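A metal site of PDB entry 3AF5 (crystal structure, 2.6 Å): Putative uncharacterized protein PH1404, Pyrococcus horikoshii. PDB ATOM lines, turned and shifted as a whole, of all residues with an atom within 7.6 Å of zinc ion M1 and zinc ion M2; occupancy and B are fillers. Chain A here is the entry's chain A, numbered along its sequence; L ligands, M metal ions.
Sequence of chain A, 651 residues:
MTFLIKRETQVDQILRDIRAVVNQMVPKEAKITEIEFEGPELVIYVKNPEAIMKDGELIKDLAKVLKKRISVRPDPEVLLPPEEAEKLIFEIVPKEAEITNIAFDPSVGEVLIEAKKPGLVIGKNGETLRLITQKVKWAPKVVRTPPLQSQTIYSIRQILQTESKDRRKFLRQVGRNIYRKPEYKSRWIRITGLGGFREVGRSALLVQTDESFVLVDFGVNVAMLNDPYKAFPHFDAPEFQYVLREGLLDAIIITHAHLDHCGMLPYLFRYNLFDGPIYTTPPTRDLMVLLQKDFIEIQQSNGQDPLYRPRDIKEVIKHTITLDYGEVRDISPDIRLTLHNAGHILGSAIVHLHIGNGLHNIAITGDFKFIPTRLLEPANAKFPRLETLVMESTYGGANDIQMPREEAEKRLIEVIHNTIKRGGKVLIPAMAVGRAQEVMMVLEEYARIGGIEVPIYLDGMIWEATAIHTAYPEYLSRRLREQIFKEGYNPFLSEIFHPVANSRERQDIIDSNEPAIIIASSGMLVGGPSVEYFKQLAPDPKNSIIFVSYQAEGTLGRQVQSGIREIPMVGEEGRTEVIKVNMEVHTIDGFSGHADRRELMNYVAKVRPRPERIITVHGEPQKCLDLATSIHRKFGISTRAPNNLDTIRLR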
ATOM      1  N   VAL A 200       7.835  31.023 -19.416  1.00  0.00           N
ATOM      2  CA  VAL A 200       6.927  29.892 -19.503  1.00  0.00           C
ATOM      3  C   VAL A 200       5.945  30.117 -18.363  1.00  0.00           C
ATOM      4  O   VAL A 200       6.335  30.187 -17.210  1.00  0.00           O
ATOM      5  CB  VAL A 200       7.679  28.554 -19.298  1.00  0.00           C
ATOM      6  CG1 VAL A 200       6.680  27.416 -19.160  1.00  0.00           C
ATOM      7  CG2 VAL A 200       8.608  28.309 -20.475  1.00  0.00           C
ATOM      8  N   GLY A 201       4.664  30.245 -18.694  1.00  0.00           N
ATOM      9  CA  GLY A 201       3.667  30.464 -17.658  1.00  0.00           C
ATOM     10  C   GLY A 201       2.696  31.568 -18.042  1.00  0.00           C
ATOM     11  O   GLY A 201       3.053  32.488 -18.801  1.00  0.00           O
ATOM     12  N   ARG A 202       1.472  31.475 -17.541  1.00  0.00           N
ATOM     13  CA  ARG A 202       0.422  32.461 -17.792  1.00  0.00           C
ATOM     14  C   ARG A 202       0.296  32.955 -19.226  1.00  0.00           C
ATOM     15  O   ARG A 202       0.208  34.163 -19.465  1.00  0.00           O
ATOM     16  CB  ARG A 202       0.612  33.680 -16.878  1.00  0.00           C
ATOM     17  CG  ARG A 202       1.933  34.428 -17.105  1.00  0.00           C
ATOM     18  CD  ARG A 202       1.994  35.748 -16.356  1.00  0.00           C
ATOM     19  NE  ARG A 202       3.314  36.344 -16.453  1.00  0.00           N
ATOM     20  CZ  ARG A 202       3.719  37.398 -15.752  1.00  0.00           C
ATOM     21  NH1 ARG A 202       2.878  37.974 -14.907  1.00  0.00           N
ATOM     22  NH2 ARG A 202       4.954  37.863 -15.876  1.00  0.00           N
ATOM     23  N   SER A 203       0.273  32.030 -20.189  1.00  0.00           N
ATOM     24  CA  SER A 203       0.118  32.427 -21.582  1.00  0.00           C
ATOM     25  C   SER A 203      -1.179  33.213 -21.788  1.00  0.00           C
ATOM     26  O   SER A 203      -2.269  32.769 -21.407  1.00  0.00           O
ATOM     27  CB  SER A 203       0.115  31.195 -22.498  1.00  0.00           C
ATOM     28  OG  SER A 203       1.417  30.671 -22.672  1.00  0.00           O
ATOM     29  N   ASP A 217      -5.754  32.016 -25.143  1.00  0.00           N
ATOM     30  CA  ASP A 217      -5.223  31.472 -23.892  1.00  0.00           C
ATOM     31  C   ASP A 217      -5.312  32.495 -22.778  1.00  0.00           C
ATOM     32  O   ASP A 217      -5.419  33.707 -23.026  1.00  0.00           O
ATOM     33  CB  ASP A 217      -3.786  30.971 -24.033  1.00  0.00           C
ATOM     34  CG  ASP A 217      -3.709  29.576 -24.647  1.00  0.00           C
ATOM     35  OD1 ASP A 217      -4.788  28.970 -24.861  1.00  0.00           O
ATOM     36  OD2 ASP A 217      -2.593  29.077 -24.918  1.00  0.00           O
ATOM     37  N   THR A 255      -5.920  26.947 -26.418  1.00  0.00           N
ATOM     38  CA  THR A 255      -5.151  25.977 -27.189  1.00  0.00           C
ATOM     39  C   THR A 255      -5.200  24.571 -26.590  1.00  0.00           C
ATOM     40  O   THR A 255      -5.335  23.591 -27.336  1.00  0.00           O
ATOM     41  CB  THR A 255      -3.680  26.388 -27.308  1.00  0.00           C
ATOM     42  OG1 THR A 255      -3.084  26.396 -26.010  1.00  0.00           O
ATOM     43  CG2 THR A 255      -3.566  27.754 -27.948  1.00  0.00           C
ATOM     44  N   HIS A 256      -5.059  24.471 -25.273  1.00  0.00           N
ATOM     45  CA  HIS A 256      -5.141  23.179 -24.591  1.00  0.00           C
ATOM     46  C   HIS A 256      -5.414  23.294 -23.090  1.00  0.00           C
ATOM     47  O   HIS A 256      -5.327  24.368 -22.495  1.00  0.00           O
ATOM     48  CB  HIS A 256      -3.892  22.334 -24.843  1.00  0.00           C
ATOM     49  CG  HIS A 256      -2.628  22.892 -24.269  1.00  0.00           C
ATOM     50  ND1 HIS A 256      -2.035  24.047 -24.754  1.00  0.00           N
ATOM     51  CD2 HIS A 256      -1.774  22.399 -23.341  1.00  0.00           C
ATOM     52  CE1 HIS A 256      -0.881  24.230 -24.144  1.00  0.00           C
ATOM     53  NE2 HIS A 256      -0.696  23.240 -23.281  1.00  0.00           N
ATOM     54  N   ALA A 257      -5.751  22.163 -22.487  1.00  0.00           N
ATOM     55  CA  ALA A 257      -6.131  22.101 -21.088  1.00  0.00           C
ATOM     56  C   ALA A 257      -5.167  22.479 -19.970  1.00  0.00           C
ATOM     57  O   ALA A 257      -5.622  22.702 -18.850  1.00  0.00           O
ATOM     58  CB  ALA A 257      -6.710  20.740 -20.803  1.00  0.00           C
ATOM     59  N   HIS A 258      -3.866  22.572 -20.217  1.00  0.00           N
ATOM     60  CA  HIS A 258      -2.966  22.918 -19.118  1.00  0.00           C
ATOM     61  C   HIS A 258      -3.224  24.263 -18.388  1.00  0.00           C
ATOM     62  O   HIS A 258      -3.670  25.245 -18.995  1.00  0.00           O
ATOM     63  CB  HIS A 258      -1.514  22.815 -19.598  1.00  0.00           C
ATOM     64  CG  HIS A 258      -1.056  21.401 -19.754  1.00  0.00           C
ATOM     65  ND1 HIS A 258      -0.230  20.995 -20.785  1.00  0.00           N
ATOM     66  CD2 HIS A 258      -1.287  20.303 -19.004  1.00  0.00           C
ATOM     67  CE1 HIS A 258       0.021  19.702 -20.653  1.00  0.00           C
ATOM     68  NE2 HIS A 258      -0.611  19.257 -19.587  1.00  0.00           N
ATOM     69  N   LEU A 259      -2.949  24.287 -17.089  1.00  0.00           N
ATOM     70  CA  LEU A 259      -3.210  25.477 -16.281  1.00  0.00           C
ATOM     71  C   LEU A 259      -2.486  26.759 -16.697  1.00  0.00           C
ATOM     72  O   LEU A 259      -2.989  27.848 -16.447  1.00  0.00           O
ATOM     73  CB  LEU A 259      -2.942  25.181 -14.804  1.00  0.00           C
ATOM     74  CG  LEU A 259      -3.902  24.249 -14.051  1.00  0.00           C
ATOM     75  CD1 LEU A 259      -3.416  24.088 -12.616  1.00  0.00           C
ATOM     76  CD2 LEU A 259      -5.318  24.798 -14.044  1.00  0.00           C
ATOM     77  N   ASP A 260      -1.321  26.642 -17.312  1.00  0.00           N
ATOM     78  CA  ASP A 260      -0.647  27.862 -17.721  1.00  0.00           C
ATOM     79  C   ASP A 260      -1.131  28.348 -19.081  1.00  0.00           C
ATOM     80  O   ASP A 260      -0.511  29.190 -19.706  1.00  0.00           O
ATOM     81  CB  ASP A 260       0.883  27.689 -17.712  1.00  0.00           C
ATOM     82  CG  ASP A 260       1.375  26.820 -18.831  1.00  0.00           C
ATOM     83  OD1 ASP A 260       2.097  27.348 -19.703  1.00  0.00           O
ATOM     84  OD2 ASP A 260       1.043  25.614 -18.826  1.00  0.00           O
ATOM     85  N   HIS A 261      -2.264  27.808 -19.516  1.00  0.00           N
ATOM     86  CA  HIS A 261      -2.874  28.227 -20.771  1.00  0.00           C
ATOM     87  C   HIS A 261      -4.357  28.504 -20.587  1.00  0.00           C
ATOM     88  O   HIS A 261      -4.955  29.228 -21.375  1.00  0.00           O
ATOM     89  CB  HIS A 261      -2.680  27.163 -21.850  1.00  0.00           C
ATOM     90  CG  HIS A 261      -1.269  27.059 -22.327  1.00  0.00           C
ATOM     91  ND1 HIS A 261      -0.784  27.792 -23.385  1.00  0.00           N
ATOM     92  CD2 HIS A 261      -0.222  26.357 -21.844  1.00  0.00           C
ATOM     93  CE1 HIS A 261       0.505  27.547 -23.543  1.00  0.00           C
ATOM     94  NE2 HIS A 261       0.875  26.681 -22.621  1.00  0.00           N
ATOM     95  N   HIS A 344       0.185  17.750 -28.689  1.00  0.00           N
ATOM     96  CA  HIS A 344       0.787  17.997 -27.380  1.00  0.00           C
ATOM     97  C   HIS A 344       0.160  17.115 -26.287  1.00  0.00           C
ATOM     98  O   HIS A 344       0.873  16.428 -25.559  1.00  0.00           O
ATOM     99  CB  HIS A 344       0.612  19.470 -27.047  1.00  0.00           C
ATOM    100  CG  HIS A 344       1.152  19.861 -25.710  1.00  0.00           C
ATOM    101  ND1 HIS A 344       2.473  19.673 -25.361  1.00  0.00           N
ATOM    102  CD2 HIS A 344       0.565  20.465 -24.660  1.00  0.00           C
ATOM    103  CE1 HIS A 344       2.678  20.142 -24.152  1.00  0.00           C
ATOM    104  NE2 HIS A 344       1.529  20.629 -23.700  1.00  0.00           N
ATOM    105  N   ILE A 345      -1.160  17.170 -26.172  1.00  0.00           N
ATOM    106  CA  ILE A 345      -1.910  16.345 -25.222  1.00  0.00           C
ATOM    107  C   ILE A 345      -3.301  16.222 -25.830  1.00  0.00           C
ATOM    108  O   ILE A 345      -3.633  16.952 -26.766  1.00  0.00           O
ATOM    109  CB  ILE A 345      -2.075  16.992 -23.802  1.00  0.00           C
ATOM    110  CG1 ILE A 345      -3.042  18.179 -23.887  1.00  0.00           C
ATOM    111  CG2 ILE A 345      -0.701  17.389 -23.216  1.00  0.00           C
ATOM    112  CD1 ILE A 345      -3.347  18.806 -22.543  1.00  0.00           C
ATOM    113  N   SER A 348      -5.234  19.070 -27.730  1.00  0.00           N
ATOM    114  CA  SER A 348      -4.421  20.274 -27.945  1.00  0.00           C
ATOM    115  C   SER A 348      -4.540  20.783 -29.376  1.00  0.00           C
ATOM    116  O   SER A 348      -4.435  19.991 -30.327  1.00  0.00           O
ATOM    117  CB  SER A 348      -2.954  20.013 -27.590  1.00  0.00           C
ATOM    118  OG  SER A 348      -2.361  19.070 -28.456  1.00  0.00           O
ATOM    119  N   GLY A 366       0.516  27.444 -29.490  1.00  0.00           N
ATOM    120  CA  GLY A 366       0.227  26.902 -28.175  1.00  0.00           C
ATOM    121  C   GLY A 366       1.394  25.963 -27.940  1.00  0.00           C
ATOM    122  O   GLY A 366       2.515  26.232 -28.385  1.00  0.00           O
ATOM    123  N   ASP A 367       1.205  24.851 -27.245  1.00  0.00           N
ATOM    124  CA  ASP A 367       2.329  23.937 -27.105  1.00  0.00           C
ATOM    125  C   ASP A 367       2.089  22.885 -28.175  1.00  0.00           C
ATOM    126  O   ASP A 367       0.943  22.537 -28.477  1.00  0.00           O
ATOM    127  CB  ASP A 367       2.336  23.301 -25.726  1.00  0.00           C
ATOM    128  CG  ASP A 367       2.645  24.298 -24.634  1.00  0.00           C
ATOM    129  OD1 ASP A 367       2.396  23.977 -23.464  1.00  0.00           O
ATOM    130  OD2 ASP A 367       3.123  25.396 -24.953  1.00  0.00           O
ATOM    131  N   PHE A 368       3.168  22.404 -28.793  1.00  0.00           N
ATOM    132  CA  PHE A 368       3.005  21.408 -29.832  1.00  0.00           C
ATOM    133  C   PHE A 368       4.157  20.441 -29.889  1.00  0.00           C
ATOM    134  O   PHE A 368       5.258  20.706 -29.382  1.00  0.00           O
ATOM    135  CB  PHE A 368       2.818  22.080 -31.212  1.00  0.00           C
ATOM    136  CG  PHE A 368       4.078  22.646 -31.794  1.00  0.00           C
ATOM    137  CD1 PHE A 368       4.595  23.847 -31.354  1.00  0.00           C
ATOM    138  CD2 PHE A 368       4.747  21.961 -32.810  1.00  0.00           C
ATOM    139  CE1 PHE A 368       5.773  24.377 -31.893  1.00  0.00           C
ATOM    140  CE2 PHE A 368       5.933  22.465 -33.366  1.00  0.00           C
ATOM    141  CZ  PHE A 368       6.446  23.678 -32.910  1.00  0.00           C
ATOM    142  N   GLU A 392       5.918  28.331 -29.717  1.00  0.00           N
ATOM    143  CA  GLU A 392       6.544  28.128 -28.431  1.00  0.00           C
ATOM    144  C   GLU A 392       8.050  27.891 -28.534  1.00  0.00           C
ATOM    145  O   GLU A 392       8.568  27.498 -29.585  1.00  0.00           O
ATOM    146  CB  GLU A 392       5.897  26.930 -27.721  1.00  0.00           C
ATOM    147  CG  GLU A 392       6.151  25.571 -28.403  1.00  0.00           C
ATOM    148  CD  GLU A 392       6.321  24.436 -27.383  1.00  0.00           C
ATOM    149  OE1 GLU A 392       7.305  24.466 -26.612  1.00  0.00           O
ATOM    150  OE2 GLU A 392       5.464  23.533 -27.332  1.00  0.00           O
ATOM    151  N   THR A 394       9.789  26.408 -25.579  1.00  0.00           N
ATOM    152  CA  THR A 394      10.165  25.678 -24.371  1.00  0.00           C
ATOM    153  C   THR A 394      11.558  25.064 -24.490  1.00  0.00           C
ATOM    154  O   THR A 394      12.322  25.094 -23.536  1.00  0.00           O
ATOM    155  CB  THR A 394       9.153  24.573 -24.043  1.00  0.00           C
ATOM    156  OG1 THR A 394       7.835  25.117 -24.070  1.00  0.00           O
ATOM    157  CG2 THR A 394       9.427  24.034 -22.649  1.00  0.00           C
ATOM    158  N   VAL A 433      -2.941  15.321 -16.739  1.00  0.00           N
ATOM    159  CA  VAL A 433      -3.096  15.143 -18.182  1.00  0.00           C
ATOM    160  C   VAL A 433      -1.764  15.443 -18.850  1.00  0.00           C
ATOM    161  O   VAL A 433      -1.121  16.461 -18.557  1.00  0.00           O
ATOM    162  CB  VAL A 433      -4.121  16.128 -18.761  1.00  0.00           C
ATOM    163  CG1 VAL A 433      -4.415  15.754 -20.196  1.00  0.00           C
ATOM    164  CG2 VAL A 433      -5.384  16.113 -17.931  1.00  0.00           C
ATOM    165  N   ARG A 435       2.028  13.882 -19.606  1.00  0.00           N
ATOM    166  CA  ARG A 435       3.029  12.846 -19.446  1.00  0.00           C
ATOM    167  C   ARG A 435       2.482  11.603 -18.739  1.00  0.00           C
ATOM    168  O   ARG A 435       2.955  10.498 -18.972  1.00  0.00           O
ATOM    169  CB  ARG A 435       4.250  13.356 -18.654  1.00  0.00           C
ATOM    170  CG  ARG A 435       5.133  14.423 -19.326  1.00  0.00           C
ATOM    171  CD  ARG A 435       5.293  14.257 -20.831  1.00  0.00           C
ATOM    172  NE  ARG A 435       4.191  14.914 -21.529  1.00  0.00           N
ATOM    173  CZ  ARG A 435       3.627  14.486 -22.651  1.00  0.00           C
ATOM    174  NH1 ARG A 435       4.078  13.381 -23.239  1.00  0.00           N
ATOM    175  NH2 ARG A 435       2.610  15.161 -23.170  1.00  0.00           N
ATOM    176  N   GLY A 593       6.248  16.439 -24.079  1.00  0.00           N
ATOM    177  CA  GLY A 593       5.142  16.760 -24.959  1.00  0.00           C
ATOM    178  C   GLY A 593       5.494  17.976 -25.779  1.00  0.00           C
ATOM    179  O   GLY A 593       4.680  18.467 -26.552  1.00  0.00           O
ATOM    180  N   HIS A 594       6.706  18.496 -25.590  1.00  0.00           N
ATOM    181  CA  HIS A 594       7.165  19.681 -26.330  1.00  0.00           C
ATOM    182  C   HIS A 594       8.136  19.312 -27.425  1.00  0.00           C
ATOM    183  O   HIS A 594       8.973  18.430 -27.249  1.00  0.00           O
ATOM    184  CB  HIS A 594       7.891  20.657 -25.401  1.00  0.00           C
ATOM    185  CG  HIS A 594       7.024  21.295 -24.379  1.00  0.00           C
ATOM    186  ND1 HIS A 594       6.071  22.250 -24.695  1.00  0.00           N
ATOM    187  CD2 HIS A 594       6.958  21.128 -23.030  1.00  0.00           C
ATOM    188  CE1 HIS A 594       5.473  22.643 -23.589  1.00  0.00           C
ATOM    189  NE2 HIS A 594       5.988  21.977 -22.572  1.00  0.00           N
ATOM    190  N   HIS A 618       6.668  31.623 -25.135  1.00  0.00           N
ATOM    191  CA  HIS A 618       6.582  30.475 -24.254  1.00  0.00           C
ATOM    192  C   HIS A 618       7.898  29.702 -24.130  1.00  0.00           C
ATOM    193  O   HIS A 618       8.020  28.585 -24.621  1.00  0.00           O
ATOM    194  CB  HIS A 618       5.466  29.569 -24.765  1.00  0.00           C
ATOM    195  CG  HIS A 618       5.064  28.480 -23.826  1.00  0.00           C
ATOM    196  ND1 HIS A 618       5.925  27.470 -23.441  1.00  0.00           N
ATOM    197  CD2 HIS A 618       3.880  28.211 -23.230  1.00  0.00           C
ATOM    198  CE1 HIS A 618       5.275  26.619 -22.663  1.00  0.00           C
ATOM    199  NE2 HIS A 618       4.036  27.050 -22.516  1.00  0.00           N
HETATM  200  S1  LIG L   1       3.940  23.559 -20.011  1.00  0.00           S
HETATM  201  O1  LIG L   1       4.713  23.185 -18.810  1.00  0.00           O
HETATM  202  O2  LIG L   1       2.511  23.497 -19.696  1.00  0.00           O
HETATM  203  O3  LIG L   1       4.312  24.915 -20.429  1.00  0.00           O
HETATM  204  O4  LIG L   1       4.229  22.603 -21.108  1.00  0.00           O
HETATM  205 ZN    ZN M   1       2.531  25.584 -21.856  1.00  0.00          ZN
HETATM  206 ZN    ZN M   2       0.982  22.251 -22.154  1.00  0.00          ZN
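The nearest printed residue that does not touch zinc ion M2 is His 261 (4.3 Å).
Of the 25 residues printed, 4 come within 4 Å of zinc ion M1.
NE2 of His 261 is bound to zinc ion M1, 2.1 Å away. A ring nitrogen (NE2) of His 618 binds zinc ion M1. The side-chain carboxylate (OD1) of Asp 367 binds zinc ion M1 (2.3 Å). O3 of the ligand binds zinc ion M1 (2.4 Å). Zinc ion M1 has four donor atoms within binding distance. Slightly farther from zinc ion M1 lies OD1 of Asp 260 (2.8 Å).
O of His 618 lies within hydrogen-bond range of N of Thr 394 (3.0 Å). O of Asp 260 is in hydrogen-bond range of N of Ser 203, 3.0 Å away. The backbone NH of His 344 lies within hydrogen-bond range of the side-chain hydroxyl of Ser 348 (2.9 Å). A ring nitrogen (NE2) of His 618 lies close to the side-chain carboxylate of Asp 260. O of His 344 sits at hydrogen-bond distance from NH2 of Arg 435 (3.2 Å). A ring nitrogen (NE2) of His 258 sits at hydrogen-bond distance from the backbone carbonyl oxygen (O) of Val 433 (3.0 Å). A ring nitrogen (NE2) of His 261 sits close to the side-chain carboxylate (OD1) of Asp 260, at 3.2 Å. A ring nitrogen (ND1) of His 344 is in hydrogen-bond range of the backbone carbonyl oxygen (O) of Gly 593 (2.8 Å).
Zinc ion M2 is bound by a ring nitrogen (ND1) of His 258 (2.2 Å), a ring nitrogen (NE2) of His 256 (2.3 Å), a ring nitrogen (NE2) of His 344 (2.3 Å) and the side-chain carboxylate of Asp 367 (2.6 Å).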
